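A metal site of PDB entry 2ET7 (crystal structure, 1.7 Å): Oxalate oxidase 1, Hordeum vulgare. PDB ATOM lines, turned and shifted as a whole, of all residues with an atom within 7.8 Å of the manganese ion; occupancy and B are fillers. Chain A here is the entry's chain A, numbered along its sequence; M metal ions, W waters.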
ATOM      1  N   VAL A  56      29.578  35.541 -33.916  1.00  0.00           N
ATOM      2  CA  VAL A  56      28.482  35.754 -32.984  1.00  0.00           C
ATOM      3  C   VAL A  56      28.364  37.232 -32.677  1.00  0.00           C
ATOM      4  O   VAL A  56      29.354  37.886 -32.301  1.00  0.00           O
ATOM      5  CB  VAL A  56      28.704  34.971 -31.661  1.00  0.00           C
ATOM      6  CG1 VAL A  56      27.549  35.244 -30.664  1.00  0.00           C
ATOM      7  CG2 VAL A  56      28.884  33.469 -31.932  1.00  0.00           C
ATOM      8  N   VAL A  77      23.958  34.813 -35.071  1.00  0.00           N
ATOM      9  CA  VAL A  77      25.180  34.130 -35.523  1.00  0.00           C
ATOM     10  C   VAL A  77      25.118  34.050 -37.037  1.00  0.00           C
ATOM     11  O   VAL A  77      24.109  33.592 -37.584  1.00  0.00           O
ATOM     12  CB  VAL A  77      25.359  32.740 -34.888  1.00  0.00           C
ATOM     13  CG1 VAL A  77      26.749  32.183 -35.199  1.00  0.00           C
ATOM     14  CG2 VAL A  77      25.151  32.820 -33.345  1.00  0.00           C
ATOM     15  N   ASN A  85      29.699  27.246 -36.003  1.00  0.00           N
ATOM     16  CA  ASN A  85      29.679  27.701 -34.621  1.00  0.00           C
ATOM     17  C   ASN A  85      29.999  26.429 -33.837  1.00  0.00           C
ATOM     18  O   ASN A  85      29.136  25.528 -33.703  1.00  0.00           O
ATOM     19  CB  ASN A  85      28.302  28.248 -34.251  1.00  0.00           C
ATOM     20  CG  ASN A  85      28.299  29.054 -32.966  1.00  0.00           C
ATOM     21  OD1 ASN A  85      29.366  29.416 -32.429  1.00  0.00           O
ATOM     22  ND2 ASN A  85      27.112  29.365 -32.473  1.00  0.00           N
ATOM     23  N   PRO A  86      31.254  26.308 -33.375  1.00  0.00           N
ATOM     24  CA  PRO A  86      31.803  25.008 -32.965  1.00  0.00           C
ATOM     25  C   PRO A  86      31.163  24.472 -31.704  1.00  0.00           C
ATOM     26  O   PRO A  86      30.527  25.260 -30.990  1.00  0.00           O
ATOM     27  CB  PRO A  86      33.298  25.303 -32.727  1.00  0.00           C
ATOM     28  CG  PRO A  86      33.358  26.728 -32.431  1.00  0.00           C
ATOM     29  CD  PRO A  86      32.249  27.392 -33.191  1.00  0.00           C
ATOM     30  N   PRO A  87      31.303  23.156 -31.442  1.00  0.00           N
ATOM     31  CA  PRO A  87      30.770  22.570 -30.213  1.00  0.00           C
ATOM     32  C   PRO A  87      31.006  23.492 -29.003  1.00  0.00           C
ATOM     33  O   PRO A  87      32.153  23.880 -28.706  1.00  0.00           O
ATOM     34  CB  PRO A  87      31.544  21.272 -30.087  1.00  0.00           C
ATOM     35  CG  PRO A  87      31.735  20.839 -31.524  1.00  0.00           C
ATOM     36  CD  PRO A  87      31.989  22.130 -32.271  1.00  0.00           C
ATOM     37  N   HIS A  88      29.916  23.845 -28.336  1.00  0.00           N
ATOM     38  CA  HIS A  88      30.010  24.742 -27.194  1.00  0.00           C
ATOM     39  C   HIS A  88      28.834  24.519 -26.256  1.00  0.00           C
ATOM     40  O   HIS A  88      27.889  23.819 -26.612  1.00  0.00           O
ATOM     41  CB  HIS A  88      30.076  26.221 -27.644  1.00  0.00           C
ATOM     42  CG  HIS A  88      28.796  26.732 -28.255  1.00  0.00           C
ATOM     43  ND1 HIS A  88      28.458  26.509 -29.576  1.00  0.00           N
ATOM     44  CD2 HIS A  88      27.772  27.450 -27.722  1.00  0.00           C
ATOM     45  CE1 HIS A  88      27.287  27.062 -29.828  1.00  0.00           C
ATOM     46  NE2 HIS A  88      26.849  27.645 -28.718  1.00  0.00           N
ATOM     47  N   ILE A  89      28.913  25.139 -25.084  1.00  0.00           N
ATOM     48  CA  ILE A  89      27.898  25.019 -24.040  1.00  0.00           C
ATOM     49  C   ILE A  89      27.560  26.421 -23.516  1.00  0.00           C
ATOM     50  O   ILE A  89      28.441  27.290 -23.451  1.00  0.00           O
ATOM     51  CB  ILE A  89      28.491  24.204 -22.897  1.00  0.00           C
ATOM     52  CG1 ILE A  89      28.491  22.727 -23.296  1.00  0.00           C
ATOM     53  CG2 ILE A  89      27.739  24.448 -21.587  1.00  0.00           C
ATOM     54  CD1 ILE A  89      29.274  21.833 -22.405  1.00  0.00           C
ATOM     55  N   HIS A  90      26.290  26.645 -23.155  1.00  0.00           N
ATOM     56  CA  HIS A  90      25.909  27.853 -22.397  1.00  0.00           C
ATOM     57  C   HIS A  90      25.666  27.387 -20.976  1.00  0.00           C
ATOM     58  O   HIS A  90      24.718  26.651 -20.735  1.00  0.00           O
ATOM     59  CB  HIS A  90      24.637  28.483 -22.971  1.00  0.00           C
ATOM     60  CG  HIS A  90      24.772  28.815 -24.402  1.00  0.00           C
ATOM     61  ND1 HIS A  90      25.670  29.763 -24.843  1.00  0.00           N
ATOM     62  CD2 HIS A  90      24.217  28.273 -25.509  1.00  0.00           C
ATOM     63  CE1 HIS A  90      25.627  29.823 -26.172  1.00  0.00           C
ATOM     64  NE2 HIS A  90      24.764  28.928 -26.600  1.00  0.00           N
ATOM     65  N   ALA A  93      21.966  28.911 -19.295  1.00  0.00           N
ATOM     66  CA  ALA A  93      20.680  29.165 -19.993  1.00  0.00           C
ATOM     67  C   ALA A  93      20.362  28.105 -20.998  1.00  0.00           C
ATOM     68  O   ALA A  93      21.256  27.545 -21.640  1.00  0.00           O
ATOM     69  CB  ALA A  93      20.733  30.511 -20.729  1.00  0.00           C
ATOM     70  N   GLU A  95      18.727  27.689 -24.664  1.00  0.00           N
ATOM     71  CA  GLU A  95      18.703  28.500 -25.877  1.00  0.00           C
ATOM     72  C   GLU A  95      17.542  28.066 -26.789  1.00  0.00           C
ATOM     73  O   GLU A  95      17.259  26.860 -26.925  1.00  0.00           O
ATOM     74  CB  GLU A  95      20.029  28.313 -26.619  1.00  0.00           C
ATOM     75  CG  GLU A  95      20.116  29.041 -27.942  1.00  0.00           C
ATOM     76  CD  GLU A  95      21.424  28.794 -28.635  1.00  0.00           C
ATOM     77  OE1 GLU A  95      22.364  28.211 -28.012  1.00  0.00           O
ATOM     78  OE2 GLU A  95      21.519  29.181 -29.819  1.00  0.00           O
ATOM     79  N   PHE A 129      14.896  25.426 -33.187  1.00  0.00           N
ATOM     80  CA  PHE A 129      15.533  24.392 -32.379  1.00  0.00           C
ATOM     81  C   PHE A 129      15.628  24.905 -30.943  1.00  0.00           C
ATOM     82  O   PHE A 129      15.568  26.125 -30.683  1.00  0.00           O
ATOM     83  CB  PHE A 129      16.943  24.069 -32.924  1.00  0.00           C
ATOM     84  CG  PHE A 129      17.838  25.287 -33.049  1.00  0.00           C
ATOM     85  CD1 PHE A 129      18.632  25.704 -31.968  1.00  0.00           C
ATOM     86  CD2 PHE A 129      17.916  25.994 -34.254  1.00  0.00           C
ATOM     87  CE1 PHE A 129      19.446  26.828 -32.084  1.00  0.00           C
ATOM     88  CE2 PHE A 129      18.752  27.117 -34.379  1.00  0.00           C
ATOM     89  CZ  PHE A 129      19.516  27.537 -33.278  1.00  0.00           C
ATOM     90  N   ILE A 131      17.857  24.120 -27.172  1.00  0.00           N
ATOM     91  CA  ILE A 131      19.054  23.504 -26.606  1.00  0.00           C
ATOM     92  C   ILE A 131      19.025  23.668 -25.094  1.00  0.00           C
ATOM     93  O   ILE A 131      19.178  24.783 -24.610  1.00  0.00           O
ATOM     94  CB  ILE A 131      20.363  24.172 -27.106  1.00  0.00           C
ATOM     95  CG1 ILE A 131      20.340  24.421 -28.628  1.00  0.00           C
ATOM     96  CG2 ILE A 131      21.585  23.415 -26.581  1.00  0.00           C
ATOM     97  CD1 ILE A 131      20.730  23.316 -29.435  1.00  0.00           C
ATOM     98  N   LEU A 135      24.168  21.847 -22.193  1.00  0.00           N
ATOM     99  CA  LEU A 135      24.454  20.752 -23.121  1.00  0.00           C
ATOM    100  C   LEU A 135      25.292  21.191 -24.310  1.00  0.00           C
ATOM    101  O   LEU A 135      25.106  22.283 -24.847  1.00  0.00           O
ATOM    102  CB  LEU A 135      23.174  20.053 -23.590  1.00  0.00           C
ATOM    103  CG  LEU A 135      22.352  19.391 -22.482  1.00  0.00           C
ATOM    104  CD1 LEU A 135      21.160  18.697 -23.124  1.00  0.00           C
ATOM    105  CD2 LEU A 135      23.196  18.396 -21.643  1.00  0.00           C
ATOM    106  N   MET A 136      26.198  20.319 -24.734  1.00  0.00           N
ATOM    107  CA  MET A 136      27.032  20.631 -25.890  1.00  0.00           C
ATOM    108  C   MET A 136      26.192  20.678 -27.174  1.00  0.00           C
ATOM    109  O   MET A 136      25.267  19.877 -27.357  1.00  0.00           O
ATOM    110  CB  MET A 136      28.163  19.620 -26.026  1.00  0.00           C
ATOM    111  CG  MET A 136      29.313  20.148 -26.896  1.00  0.00           C
ATOM    112  SD  MET A 136      30.629  18.945 -27.146  1.00  0.00           S
ATOM    113  CE  MET A 136      31.091  18.597 -25.428  1.00  0.00           C
ATOM    114  N   HIS A 137      26.521  21.621 -28.049  1.00  0.00           N
ATOM    115  CA  HIS A 137      25.799  21.725 -29.331  1.00  0.00           C
ATOM    116  C   HIS A 137      26.650  22.494 -30.354  1.00  0.00           C
ATOM    117  O   HIS A 137      27.636  23.142 -29.990  1.00  0.00           O
ATOM    118  CB  HIS A 137      24.427  22.391 -29.129  1.00  0.00           C
ATOM    119  CG  HIS A 137      24.510  23.768 -28.526  1.00  0.00           C
ATOM    120  ND1 HIS A 137      24.851  23.978 -27.207  1.00  0.00           N
ATOM    121  CD2 HIS A 137      24.283  24.984 -29.056  1.00  0.00           C
ATOM    122  CE1 HIS A 137      24.848  25.273 -26.961  1.00  0.00           C
ATOM    123  NE2 HIS A 137      24.494  25.910 -28.061  1.00  0.00           N
ATOM    124  N   PHE A 138      26.270  22.418 -31.613  1.00  0.00           N
ATOM    125  CA  PHE A 138      27.019  23.105 -32.675  1.00  0.00           C
ATOM    126  C   PHE A 138      26.064  23.419 -33.840  1.00  0.00           C
ATOM    127  O   PHE A 138      24.946  22.874 -33.905  1.00  0.00           O
ATOM    128  CB  PHE A 138      28.198  22.225 -33.151  1.00  0.00           C
ATOM    129  CG  PHE A 138      27.758  20.939 -33.828  1.00  0.00           C
ATOM    130  CD1 PHE A 138      27.358  20.944 -35.171  1.00  0.00           C
ATOM    131  CD2 PHE A 138      27.708  19.750 -33.099  1.00  0.00           C
ATOM    132  CE1 PHE A 138      26.924  19.747 -35.777  1.00  0.00           C
ATOM    133  CE2 PHE A 138      27.280  18.559 -33.693  1.00  0.00           C
ATOM    134  CZ  PHE A 138      26.874  18.552 -35.018  1.00  0.00           C
ATOM    135  N   GLN A 139      26.519  24.285 -34.741  1.00  0.00           N
ATOM    136  CA  GLN A 139      25.839  24.494 -36.020  1.00  0.00           C
ATOM    137  C   GLN A 139      26.906  24.519 -37.115  1.00  0.00           C
ATOM    138  O   GLN A 139      28.055  24.942 -36.871  1.00  0.00           O
ATOM    139  CB  GLN A 139      25.040  25.786 -36.044  1.00  0.00           C
ATOM    140  CG  GLN A 139      23.907  25.875 -34.996  1.00  0.00           C
ATOM    141  CD  GLN A 139      24.373  26.520 -33.703  1.00  0.00           C
ATOM    142  OE1 GLN A 139      25.370  27.258 -33.667  1.00  0.00           O
ATOM    143  NE2 GLN A 139      23.627  26.254 -32.629  1.00  0.00           N
ATOM    144  N   MET A 149      21.258  32.833 -38.096  1.00  0.00           N
ATOM    145  CA  MET A 149      20.185  32.482 -37.206  1.00  0.00           C
ATOM    146  C   MET A 149      20.098  33.559 -36.128  1.00  0.00           C
ATOM    147  O   MET A 149      21.072  34.289 -35.878  1.00  0.00           O
ATOM    148  CB  MET A 149      20.436  31.126 -36.553  1.00  0.00           C
ATOM    149  CG  MET A 149      21.640  31.130 -35.634  1.00  0.00           C
ATOM    150  SD  MET A 149      22.016  29.475 -35.037  1.00  0.00           S
ATOM    151  CE  MET A 149      23.209  29.845 -33.770  1.00  0.00           C
ATOM    152  N   VAL A 151      18.946  33.832 -32.068  1.00  0.00           N
ATOM    153  CA  VAL A 151      18.667  32.966 -30.920  1.00  0.00           C
ATOM    154  C   VAL A 151      18.372  33.788 -29.673  1.00  0.00           C
ATOM    155  O   VAL A 151      18.758  34.958 -29.565  1.00  0.00           O
ATOM    156  CB  VAL A 151      19.824  31.969 -30.653  1.00  0.00           C
ATOM    157  CG1 VAL A 151      20.045  31.079 -31.874  1.00  0.00           C
ATOM    158  CG2 VAL A 151      21.101  32.702 -30.269  1.00  0.00           C
ATOM    159  N   PHE A 153      17.781  33.397 -25.154  1.00  0.00           N
ATOM    160  CA  PHE A 153      18.166  32.573 -24.013  1.00  0.00           C
ATOM    161  C   PHE A 153      17.325  32.984 -22.810  1.00  0.00           C
ATOM    162  O   PHE A 153      16.899  34.129 -22.722  1.00  0.00           O
ATOM    163  CB  PHE A 153      19.639  32.845 -23.658  1.00  0.00           C
ATOM    164  CG  PHE A 153      20.589  32.612 -24.780  1.00  0.00           C
ATOM    165  CD1 PHE A 153      20.889  33.632 -25.700  1.00  0.00           C
ATOM    166  CD2 PHE A 153      21.225  31.376 -24.908  1.00  0.00           C
ATOM    167  CE1 PHE A 153      21.810  33.409 -26.728  1.00  0.00           C
ATOM    168  CE2 PHE A 153      22.131  31.125 -25.932  1.00  0.00           C
ATOM    169  CZ  PHE A 153      22.422  32.153 -26.860  1.00  0.00           C
ATOM    170  N   GLY A 159      26.527  32.930 -21.001  1.00  0.00           N
ATOM    171  CA  GLY A 159      27.916  32.444 -21.030  1.00  0.00           C
ATOM    172  C   GLY A 159      28.145  31.589 -22.263  1.00  0.00           C
ATOM    173  O   GLY A 159      27.199  31.004 -22.808  1.00  0.00           O
ATOM    174  N   ILE A 160      29.402  31.513 -22.704  1.00  0.00           N
ATOM    175  CA  ILE A 160      29.752  30.586 -23.758  1.00  0.00           C
ATOM    176  C   ILE A 160      31.014  29.847 -23.372  1.00  0.00           C
ATOM    177  O   ILE A 160      32.017  30.456 -23.047  1.00  0.00           O
ATOM    178  CB  ILE A 160      29.885  31.285 -25.138  1.00  0.00           C
ATOM    179  CG1 ILE A 160      30.315  30.258 -26.194  1.00  0.00           C
ATOM    180  CG2 ILE A 160      30.892  32.382 -25.104  1.00  0.00           C
ATOM    181  CD1 ILE A 160      29.521  30.321 -27.464  1.00  0.00           C
ATOM    182  N   PHE A 162      33.283  27.598 -25.293  1.00  0.00           N
ATOM    183  CA  PHE A 162      33.670  27.027 -26.576  1.00  0.00           C
ATOM    184  C   PHE A 162      34.568  25.822 -26.306  1.00  0.00           C
ATOM    185  O   PHE A 162      35.625  25.939 -25.680  1.00  0.00           O
ATOM    186  CB  PHE A 162      34.435  28.059 -27.438  1.00  0.00           C
ATOM    187  CG  PHE A 162      33.549  29.023 -28.182  1.00  0.00           C
ATOM    188  CD1 PHE A 162      33.683  30.398 -27.988  1.00  0.00           C
ATOM    189  CD2 PHE A 162      32.632  28.572 -29.137  1.00  0.00           C
ATOM    190  CE1 PHE A 162      32.887  31.309 -28.702  1.00  0.00           C
ATOM    191  CE2 PHE A 162      31.831  29.473 -29.843  1.00  0.00           C
ATOM    192  CZ  PHE A 162      31.965  30.846 -29.640  1.00  0.00           C
HETATM  193 MN    MN M   1      24.776  27.944 -28.417  1.00  0.00          MN
HETATM  194  O   HOH W   1      24.369  28.769 -30.520  1.00  0.00           O
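The backbone carbonyl oxygen (O) of Pro 86 sits at hydrogen-bond distance from a ring nitrogen (ND1) of His 88, 2.8 Å away.
O of Glu 95 sits at hydrogen-bond distance from N of Ile 131, 2.8 Å away.
The backbone carbonyl oxygen (O) of Gly 159 lies within hydrogen-bond range of a ring nitrogen (ND1) of His 90, 2.8 Å away.
A ring nitrogen (ND1) of His 137 sits at hydrogen-bond distance from the backbone carbonyl oxygen of Leu 135 (2.9 Å).
Of the 23 residues printed, 4 come within 4 Å of the manganese ion.
The nearest printed residue that does not touch the manganese ion is Gln 139 (4.7 Å).
The manganese ion is bound by a ring nitrogen (NE2) of His 90 (2.1 Å), a ring nitrogen (NE2) of His 137 (2.1 Å), a ring nitrogen (NE2) of His 88 (2.1 Å), water W1 (2.3 Å) and the side-chain carboxylate (OE1) of Glu 95 (2.5 Å).
Water W1 lies within hydrogen-bond range of OE2 of Glu 95 (3.0 Å), NE2 of Gln 139 (3.4 Å) and ND2 of Asn 85 (3.4 Å).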
